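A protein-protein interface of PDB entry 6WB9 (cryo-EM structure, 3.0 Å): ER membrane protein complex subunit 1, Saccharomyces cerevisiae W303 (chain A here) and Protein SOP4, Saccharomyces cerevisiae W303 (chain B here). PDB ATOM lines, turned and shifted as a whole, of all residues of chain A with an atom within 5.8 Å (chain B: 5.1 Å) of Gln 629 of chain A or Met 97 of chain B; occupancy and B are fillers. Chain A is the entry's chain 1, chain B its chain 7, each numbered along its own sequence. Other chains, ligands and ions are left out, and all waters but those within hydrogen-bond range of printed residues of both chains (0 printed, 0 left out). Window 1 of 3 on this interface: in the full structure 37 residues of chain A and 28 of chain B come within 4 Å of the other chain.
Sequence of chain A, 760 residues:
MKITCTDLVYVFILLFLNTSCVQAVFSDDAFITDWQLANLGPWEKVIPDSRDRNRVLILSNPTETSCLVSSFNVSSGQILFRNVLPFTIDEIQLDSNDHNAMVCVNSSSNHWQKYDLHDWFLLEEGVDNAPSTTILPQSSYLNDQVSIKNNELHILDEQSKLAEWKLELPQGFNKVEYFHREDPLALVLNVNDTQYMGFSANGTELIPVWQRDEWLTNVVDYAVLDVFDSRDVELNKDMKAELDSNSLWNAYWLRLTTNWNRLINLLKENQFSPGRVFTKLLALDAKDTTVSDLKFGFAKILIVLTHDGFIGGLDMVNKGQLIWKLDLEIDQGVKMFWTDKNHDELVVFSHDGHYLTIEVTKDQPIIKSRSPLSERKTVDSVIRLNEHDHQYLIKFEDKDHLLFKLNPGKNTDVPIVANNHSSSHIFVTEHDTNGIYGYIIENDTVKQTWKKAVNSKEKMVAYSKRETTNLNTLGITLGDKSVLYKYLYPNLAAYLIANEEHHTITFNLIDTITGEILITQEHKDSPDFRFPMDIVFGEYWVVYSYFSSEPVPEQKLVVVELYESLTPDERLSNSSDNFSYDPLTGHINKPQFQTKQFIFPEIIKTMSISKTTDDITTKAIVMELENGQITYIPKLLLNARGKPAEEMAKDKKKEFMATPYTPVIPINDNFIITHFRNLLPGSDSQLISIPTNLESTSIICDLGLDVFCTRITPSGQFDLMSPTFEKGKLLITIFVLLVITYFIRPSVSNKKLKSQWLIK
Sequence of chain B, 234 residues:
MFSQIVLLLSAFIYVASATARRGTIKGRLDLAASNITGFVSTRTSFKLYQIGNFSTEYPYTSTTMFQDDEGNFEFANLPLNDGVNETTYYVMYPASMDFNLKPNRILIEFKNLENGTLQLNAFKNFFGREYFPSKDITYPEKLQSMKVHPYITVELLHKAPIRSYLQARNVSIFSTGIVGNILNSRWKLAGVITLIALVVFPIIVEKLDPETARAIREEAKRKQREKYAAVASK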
ATOM      1  N   GLU A 602      16.518  13.508  10.839  1.00  0.00           N
ATOM      2  CA  GLU A 602      16.741  14.852  10.342  1.00  0.00           C
ATOM      3  C   GLU A 602      18.220  15.067  10.058  1.00  0.00           C
ATOM      4  O   GLU A 602      19.091  14.433  10.654  1.00  0.00           O
ATOM      5  CB  GLU A 602      16.240  15.883  11.350  1.00  0.00           C
ATOM      6  CG  GLU A 602      14.742  15.850  11.566  1.00  0.00           C
ATOM      7  CD  GLU A 602      13.972  16.071  10.286  1.00  0.00           C
ATOM      8  OE1 GLU A 602      14.395  16.922   9.479  1.00  0.00           O
ATOM      9  OE2 GLU A 602      12.940  15.397  10.086  1.00  0.00           O
ATOM     10  N   MET A 623      22.250  19.389  18.842  1.00  0.00           N
ATOM     11  CA  MET A 623      22.376  19.382  17.395  1.00  0.00           C
ATOM     12  C   MET A 623      21.352  20.330  16.796  1.00  0.00           C
ATOM     13  O   MET A 623      20.146  20.158  16.996  1.00  0.00           O
ATOM     14  CB  MET A 623      22.202  17.971  16.842  1.00  0.00           C
ATOM     15  CG  MET A 623      21.287  17.113  17.665  1.00  0.00           C
ATOM     16  SD  MET A 623      21.417  15.392  17.219  1.00  0.00           S
ATOM     17  CE  MET A 623      23.136  15.106  17.594  1.00  0.00           C
ATOM     18  N   GLU A 624      21.838  21.336  16.082  1.00  0.00           N
ATOM     19  CA  GLU A 624      20.989  22.204  15.285  1.00  0.00           C
ATOM     20  C   GLU A 624      20.819  21.569  13.914  1.00  0.00           C
ATOM     21  O   GLU A 624      21.809  21.327  13.212  1.00  0.00           O
ATOM     22  CB  GLU A 624      21.592  23.599  15.168  1.00  0.00           C
ATOM     23  CG  GLU A 624      20.775  24.541  14.334  1.00  0.00           C
ATOM     24  CD  GLU A 624      21.534  25.052  13.136  1.00  0.00           C
ATOM     25  OE1 GLU A 624      22.645  25.587  13.320  1.00  0.00           O
ATOM     26  OE2 GLU A 624      21.016  24.919  12.009  1.00  0.00           O
ATOM     27  N   LEU A 625      19.570  21.288  13.555  1.00  0.00           N
ATOM     28  CA  LEU A 625      19.206  20.585  12.339  1.00  0.00           C
ATOM     29  C   LEU A 625      19.093  21.560  11.172  1.00  0.00           C
ATOM     30  O   LEU A 625      19.112  22.779  11.342  1.00  0.00           O
ATOM     31  CB  LEU A 625      17.892  19.832  12.543  1.00  0.00           C
ATOM     32  CG  LEU A 625      17.752  19.076  13.864  1.00  0.00           C
ATOM     33  CD1 LEU A 625      16.355  18.539  14.028  1.00  0.00           C
ATOM     34  CD2 LEU A 625      18.762  17.953  13.958  1.00  0.00           C
ATOM     35  N   GLU A 626      18.968  21.005   9.965  1.00  0.00           N
ATOM     36  CA  GLU A 626      19.003  21.834   8.768  1.00  0.00           C
ATOM     37  C   GLU A 626      17.708  22.598   8.528  1.00  0.00           C
ATOM     38  O   GLU A 626      17.706  23.544   7.736  1.00  0.00           O
ATOM     39  CB  GLU A 626      19.325  20.984   7.536  1.00  0.00           C
ATOM     40  CG  GLU A 626      18.138  20.239   6.951  1.00  0.00           C
ATOM     41  CD  GLU A 626      18.329  19.902   5.487  1.00  0.00           C
ATOM     42  OE1 GLU A 626      19.423  20.174   4.949  1.00  0.00           O
ATOM     43  OE2 GLU A 626      17.385  19.366   4.871  1.00  0.00           O
ATOM     44  N   ASN A 627      16.616  22.223   9.187  1.00  0.00           N
ATOM     45  CA  ASN A 627      15.360  22.947   9.052  1.00  0.00           C
ATOM     46  C   ASN A 627      15.236  24.095  10.041  1.00  0.00           C
ATOM     47  O   ASN A 627      14.207  24.775  10.057  1.00  0.00           O
ATOM     48  CB  ASN A 627      14.171  21.993   9.208  1.00  0.00           C
ATOM     49  CG  ASN A 627      14.291  21.084  10.415  1.00  0.00           C
ATOM     50  OD1 ASN A 627      15.159  21.261  11.260  1.00  0.00           O
ATOM     51  ND2 ASN A 627      13.403  20.107  10.504  1.00  0.00           N
ATOM     52  N   GLY A 628      16.257  24.326  10.861  1.00  0.00           N
ATOM     53  CA  GLY A 628      16.241  25.359  11.861  1.00  0.00           C
ATOM     54  C   GLY A 628      15.991  24.860  13.267  1.00  0.00           C
ATOM     55  O   GLY A 628      16.291  25.578  14.223  1.00  0.00           O
ATOM     56  N   GLN A 629      15.453  23.655  13.413  1.00  0.00           N
ATOM     57  CA  GLN A 629      15.164  23.117  14.730  1.00  0.00           C
ATOM     58  C   GLN A 629      16.445  22.709  15.437  1.00  0.00           C
ATOM     59  O   GLN A 629      17.427  22.310  14.812  1.00  0.00           O
ATOM     60  CB  GLN A 629      14.230  21.916  14.623  1.00  0.00           C
ATOM     61  CG  GLN A 629      12.818  22.271  14.232  1.00  0.00           C
ATOM     62  CD  GLN A 629      11.918  21.064  14.188  1.00  0.00           C
ATOM     63  OE1 GLN A 629      12.371  19.945  13.963  1.00  0.00           O
ATOM     64  NE2 GLN A 629      10.635  21.282  14.409  1.00  0.00           N
ATOM     65  N   ILE A 630      16.430  22.821  16.760  1.00  0.00           N
ATOM     66  CA  ILE A 630      17.550  22.417  17.598  1.00  0.00           C
ATOM     67  C   ILE A 630      17.044  21.367  18.565  1.00  0.00           C
ATOM     68  O   ILE A 630      16.106  21.621  19.327  1.00  0.00           O
ATOM     69  CB  ILE A 630      18.156  23.598  18.365  1.00  0.00           C
ATOM     70  CG1 ILE A 630      18.528  24.733  17.424  1.00  0.00           C
ATOM     71  CG2 ILE A 630      19.383  23.153  19.109  1.00  0.00           C
ATOM     72  CD1 ILE A 630      19.023  25.923  18.147  1.00  0.00           C
ATOM     73  N   THR A 631      17.648  20.193  18.532  1.00  0.00           N
ATOM     74  CA  THR A 631      17.370  19.157  19.508  1.00  0.00           C
ATOM     75  C   THR A 631      18.645  18.871  20.284  1.00  0.00           C
ATOM     76  O   THR A 631      19.669  19.519  20.087  1.00  0.00           O
ATOM     77  CB  THR A 631      16.836  17.893  18.833  1.00  0.00           C
ATOM     78  OG1 THR A 631      16.377  16.974  19.829  1.00  0.00           O
ATOM     79  CG2 THR A 631      17.909  17.241  17.996  1.00  0.00           C
ATOM     80  N   ILE A 667      13.278  10.961  16.640  1.00  0.00           N
ATOM     81  CA  ILE A 667      13.394  12.368  16.999  1.00  0.00           C
ATOM     82  C   ILE A 667      12.372  12.669  18.096  1.00  0.00           C
ATOM     83  O   ILE A 667      11.161  12.693  17.862  1.00  0.00           O
ATOM     84  CB  ILE A 667      13.236  13.284  15.776  1.00  0.00           C
ATOM     85  CG1 ILE A 667      13.109  14.752  16.187  1.00  0.00           C
ATOM     86  CG2 ILE A 667      12.111  12.818  14.826  1.00  0.00           C
ATOM     87  CD1 ILE A 667      13.250  15.694  15.020  1.00  0.00           C
ATOM     88  N   ILE A 672      13.187  18.733  21.207  1.00  0.00           N
ATOM     89  CA  ILE A 672      13.269  19.874  20.299  1.00  0.00           C
ATOM     90  C   ILE A 672      13.067  21.131  21.138  1.00  0.00           C
ATOM     91  O   ILE A 672      11.949  21.431  21.562  1.00  0.00           O
ATOM     92  CB  ILE A 672      12.231  19.785  19.175  1.00  0.00           C
ATOM     93  CG1 ILE A 672      12.430  18.517  18.339  1.00  0.00           C
ATOM     94  CG2 ILE A 672      12.271  21.039  18.310  1.00  0.00           C
ATOM     95  CD1 ILE A 672      13.515  18.617  17.309  1.00  0.00           C
ATOM     96  N   THR A 674      13.521  24.241  20.230  1.00  0.00           N
ATOM     97  CA  THR A 674      12.864  25.304  19.474  1.00  0.00           C
ATOM     98  C   THR A 674      11.429  24.881  19.162  1.00  0.00           C
ATOM     99  O   THR A 674      11.052  24.593  18.027  1.00  0.00           O
ATOM    100  CB  THR A 674      13.645  25.617  18.207  1.00  0.00           C
ATOM    101  OG1 THR A 674      13.517  24.524  17.293  1.00  0.00           O
ATOM    102  CG2 THR A 674      15.096  25.816  18.533  1.00  0.00           C
ATOM    103  N   PHE A 676       7.905  25.061  18.221  1.00  0.00           N
ATOM    104  CA  PHE A 676       7.022  25.828  17.338  1.00  0.00           C
ATOM    105  C   PHE A 676       7.624  27.141  16.844  1.00  0.00           C
ATOM    106  O   PHE A 676       6.896  27.978  16.302  1.00  0.00           O
ATOM    107  CB  PHE A 676       5.660  26.123  17.993  1.00  0.00           C
ATOM    108  CG  PHE A 676       4.890  24.899  18.382  1.00  0.00           C
ATOM    109  CD1 PHE A 676       4.259  24.128  17.419  1.00  0.00           C
ATOM    110  CD2 PHE A 676       4.780  24.530  19.711  1.00  0.00           C
ATOM    111  CE1 PHE A 676       3.546  23.002  17.775  1.00  0.00           C
ATOM    112  CE2 PHE A 676       4.068  23.407  20.075  1.00  0.00           C
ATOM    113  CZ  PHE A 676       3.450  22.643  19.107  1.00  0.00           C
ATOM    114  N   ARG A 677       8.926  27.355  17.011  1.00  0.00           N
ATOM    115  CA  ARG A 677       9.558  28.593  16.593  1.00  0.00           C
ATOM    116  C   ARG A 677      10.087  28.452  15.177  1.00  0.00           C
ATOM    117  O   ARG A 677      10.668  27.426  14.815  1.00  0.00           O
ATOM    118  CB  ARG A 677      10.705  28.971  17.530  1.00  0.00           C
ATOM    119  CG  ARG A 677      10.324  29.098  18.983  1.00  0.00           C
ATOM    120  CD  ARG A 677      11.396  29.837  19.754  1.00  0.00           C
ATOM    121  NE  ARG A 677      11.187  31.278  19.719  1.00  0.00           N
ATOM    122  CZ  ARG A 677      10.804  31.998  20.766  1.00  0.00           C
ATOM    123  NH1 ARG A 677      10.604  31.411  21.933  1.00  0.00           N
ATOM    124  NH2 ARG A 677      10.631  33.305  20.648  1.00  0.00           N
ATOM    125  N   ASN A 678       9.886  29.497  14.375  1.00  0.00           N
ATOM    126  CA  ASN A 678      10.448  29.566  13.029  1.00  0.00           C
ATOM    127  C   ASN A 678      11.869  30.123  13.121  1.00  0.00           C
ATOM    128  O   ASN A 678      12.178  31.230  12.679  1.00  0.00           O
ATOM    129  CB  ASN A 678       9.571  30.420  12.128  1.00  0.00           C
ATOM    130  CG  ASN A 678       8.149  29.915  12.051  1.00  0.00           C
ATOM    131  OD1 ASN A 678       7.377  30.045  13.001  1.00  0.00           O
ATOM    132  ND2 ASN A 678       7.789  29.344  10.910  1.00  0.00           N
ATOM    133  N   LEU A 679      12.744  29.324  13.722  1.00  0.00           N
ATOM    134  CA  LEU A 679      14.132  29.718  13.894  1.00  0.00           C
ATOM    135  C   LEU A 679      14.887  29.485  12.597  1.00  0.00           C
ATOM    136  O   LEU A 679      14.776  28.420  11.985  1.00  0.00           O
ATOM    137  CB  LEU A 679      14.776  28.934  15.035  1.00  0.00           C
ATOM    138  CG  LEU A 679      16.262  29.205  15.258  1.00  0.00           C
ATOM    139  CD1 LEU A 679      16.490  30.662  15.581  1.00  0.00           C
ATOM    140  CD2 LEU A 679      16.800  28.331  16.355  1.00  0.00           C
ATOM    141  N   ARG B  43       7.061  25.617   6.715  1.00  0.00           N
ATOM    142  CA  ARG B  43       7.405  24.718   7.804  1.00  0.00           C
ATOM    143  C   ARG B  43       7.300  23.252   7.411  1.00  0.00           C
ATOM    144  O   ARG B  43       7.731  22.392   8.183  1.00  0.00           O
ATOM    145  CB  ARG B  43       6.510  24.993   9.010  1.00  0.00           C
ATOM    146  CG  ARG B  43       6.715  26.364   9.614  1.00  0.00           C
ATOM    147  CD  ARG B  43       5.799  26.598  10.798  1.00  0.00           C
ATOM    148  NE  ARG B  43       5.986  25.614  11.858  1.00  0.00           N
ATOM    149  CZ  ARG B  43       6.904  25.709  12.814  1.00  0.00           C
ATOM    150  NH1 ARG B  43       7.728  26.745  12.840  1.00  0.00           N
ATOM    151  NH2 ARG B  43       7.004  24.770  13.741  1.00  0.00           N
ATOM    152  N   THR B  44       6.735  22.949   6.246  1.00  0.00           N
ATOM    153  CA  THR B  44       6.679  21.593   5.716  1.00  0.00           C
ATOM    154  C   THR B  44       7.488  21.548   4.430  1.00  0.00           C
ATOM    155  O   THR B  44       7.213  22.305   3.494  1.00  0.00           O
ATOM    156  CB  THR B  44       5.242  21.146   5.436  1.00  0.00           C
ATOM    157  OG1 THR B  44       4.653  22.046   4.494  1.00  0.00           O
ATOM    158  CG2 THR B  44       4.409  21.141   6.707  1.00  0.00           C
ATOM    159  N   ALA B  95       8.711  15.978   5.438  1.00  0.00           N
ATOM    160  CA  ALA B  95       8.971  16.465   6.780  1.00  0.00           C
ATOM    161  C   ALA B  95       8.127  17.700   7.037  1.00  0.00           C
ATOM    162  O   ALA B  95       7.824  18.462   6.121  1.00  0.00           O
ATOM    163  CB  ALA B  95      10.451  16.796   6.976  1.00  0.00           C
ATOM    164  N   SER B  96       7.743  17.893   8.292  1.00  0.00           N
ATOM    165  CA  SER B  96       6.996  19.082   8.661  1.00  0.00           C
ATOM    166  C   SER B  96       7.293  19.415  10.109  1.00  0.00           C
ATOM    167  O   SER B  96       7.295  18.531  10.968  1.00  0.00           O
ATOM    168  CB  SER B  96       5.492  18.886   8.463  1.00  0.00           C
ATOM    169  OG  SER B  96       5.012  17.843   9.285  1.00  0.00           O
ATOM    170  N   MET B  97       7.546  20.694  10.372  1.00  0.00           N
ATOM    171  CA  MET B  97       7.744  21.155  11.737  1.00  0.00           C
ATOM    172  C   MET B  97       6.431  21.385  12.468  1.00  0.00           C
ATOM    173  O   MET B  97       6.451  21.717  13.655  1.00  0.00           O
ATOM    174  CB  MET B  97       8.576  22.437  11.737  1.00  0.00           C
ATOM    175  CG  MET B  97       9.825  22.343  10.884  1.00  0.00           C
ATOM    176  SD  MET B  97      11.023  23.641  11.217  1.00  0.00           S
ATOM    177  CE  MET B  97      10.061  25.098  10.843  1.00  0.00           C
ATOM    178  N   ASP B  98       5.298  21.221  11.789  1.00  0.00           N
ATOM    179  CA  ASP B  98       3.980  21.367  12.388  1.00  0.00           C
ATOM    180  C   ASP B  98       3.357  20.032  12.771  1.00  0.00           C
ATOM    181  O   ASP B  98       2.950  19.848  13.920  1.00  0.00           O
ATOM    182  CB  ASP B  98       3.050  22.110  11.424  1.00  0.00           C
ATOM    183  CG  ASP B  98       3.502  23.522  11.152  1.00  0.00           C
ATOM    184  OD1 ASP B  98       3.927  24.203  12.107  1.00  0.00           O
ATOM    185  OD2 ASP B  98       3.433  23.951   9.982  1.00  0.00           O
ATOM    186  N   PHE B  99       3.273  19.094  11.831  1.00  0.00           N
ATOM    187  CA  PHE B  99       2.536  17.857  12.033  1.00  0.00           C
ATOM    188  C   PHE B  99       3.439  16.641  11.894  1.00  0.00           C
ATOM    189  O   PHE B  99       4.441  16.667  11.176  1.00  0.00           O
ATOM    190  CB  PHE B  99       1.386  17.710  11.027  1.00  0.00           C
ATOM    191  CG  PHE B  99       1.076  18.957  10.256  1.00  0.00           C
ATOM    192  CD1 PHE B  99       0.197  19.897  10.762  1.00  0.00           C
ATOM    193  CD2 PHE B  99       1.639  19.173   9.006  1.00  0.00           C
ATOM    194  CE1 PHE B  99      -0.100  21.040  10.050  1.00  0.00           C
ATOM    195  CE2 PHE B  99       1.348  20.316   8.292  1.00  0.00           C
ATOM    196  CZ  PHE B  99       0.477  21.250   8.815  1.00  0.00           C
ATOM    197  N   GLN B 167       2.491  17.893  15.894  1.00  0.00           N
ATOM    198  CA  GLN B 167       3.713  17.259  16.381  1.00  0.00           C
ATOM    199  C   GLN B 167       3.831  17.299  17.898  1.00  0.00           C
ATOM    200  O   GLN B 167       4.500  16.430  18.472  1.00  0.00           O
ATOM    201  CB  GLN B 167       4.937  17.907  15.731  1.00  0.00           C
ATOM    202  CG  GLN B 167       6.130  16.969  15.596  1.00  0.00           C
ATOM    203  CD  GLN B 167       7.191  17.491  14.646  1.00  0.00           C
ATOM    204  OE1 GLN B 167       6.956  18.438  13.902  1.00  0.00           O
ATOM    205  NE2 GLN B 167       8.366  16.873  14.669  1.00  0.00           N
ATOM    206  N   ARG B 169       5.113  19.549  20.470  1.00  0.00           N
ATOM    207  CA  ARG B 169       6.413  19.764  21.099  1.00  0.00           C
ATOM    208  C   ARG B 169       6.288  19.959  22.604  1.00  0.00           C
ATOM    209  O   ARG B 169       7.120  19.463  23.371  1.00  0.00           O
ATOM    210  CB  ARG B 169       7.102  20.970  20.469  1.00  0.00           C
ATOM    211  CG  ARG B 169       8.415  20.641  19.804  1.00  0.00           C
ATOM    212  CD  ARG B 169       8.212  19.695  18.644  1.00  0.00           C
ATOM    213  NE  ARG B 169       8.442  20.358  17.371  1.00  0.00           N
ATOM    214  CZ  ARG B 169       7.516  21.037  16.709  1.00  0.00           C
ATOM    215  NH1 ARG B 169       6.292  21.143  17.198  1.00  0.00           N
ATOM    216  NH2 ARG B 169       7.815  21.614  15.559  1.00  0.00           N
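The side-chain amide nitrogen (NE2) of Gln 629 of chain A lies close to the guanidinium group (NH2) of Arg 169 of chain B, at 3.1 Å. NH1 of Arg 43 of chain B sits close to ND2 of Asn 678 of chain A (3.2 Å). O of Asn 627 of chain A sits close to SD of Met 97 of chain B (3.6 Å).
ND2 of Asn 627 of chain A is in hydrogen-bond range of OE1 of Glu 602 of chain A. OD1 of Asn 627 of chain A lies within hydrogen-bond range of N of Gln 629 of chain A (3.2 Å). O of Arg 43 of chain B is in hydrogen-bond range of N of Met 97 of chain B (2.8 Å). OD1 of Asp 98 of chain B lies within salt-bridge range of NE of Arg 43 of chain B, at 2.5 Å. The side-chain amide oxygen (OE1) of Gln 167 of chain B lies close to the backbone carbonyl oxygen (O) of Met 97 of chain B (3.3 Å).
Gln 629 of chain A touches Met 97 of chain B. CB of Ile 672 of chain A touches CG of Arg 169 of chain B, at 3.96 Å. Phe 676 of chain A touches Arg 43 of chain B (CA to NH2, 3.7 Å). Phe 676 of chain A touches Arg 169 of chain B. Arg 677 of chain A touches Arg 43 of chain B (O to NH1, 3.6 Å).
Of chain B, only Met 97 and Arg 169 come within 4 Å of Gln 629 of chain A. Of the printed residues of chain A, Met 97 of chain B touches Asn 627 (3.6 Å) and Gln 629 (3.6 Å). Printed residues of chain A within 4 Å of Arg 169 of chain B: Gln 629, Ile 672 and Phe 676. Of the printed residues of chain B, Asn 678 of chain A touches Arg 43. Ile 630 of chain A touches none of the printed residues of chain B. The nearest residue of chain A that does not touch Met 97 of chain B is Arg 677 of chain A (4.6 Å). The nearest printed residue of chain B that does not touch Ile 672 of chain A is Gln 167 of chain B (5.7 Å).
Of the 17 printed residues of chain A, 6 touch a printed residue of chain B. Hydrophobic or aromatic side chains of chain A within 4 Å of the printed part of chain B: Ile 672 and Phe 676. Of the 9 printed residues of chain B, 3 touch a printed residue of chain A. Hydrophobic or aromatic side chains of chain B that line the printed part of chain A: Met 97.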
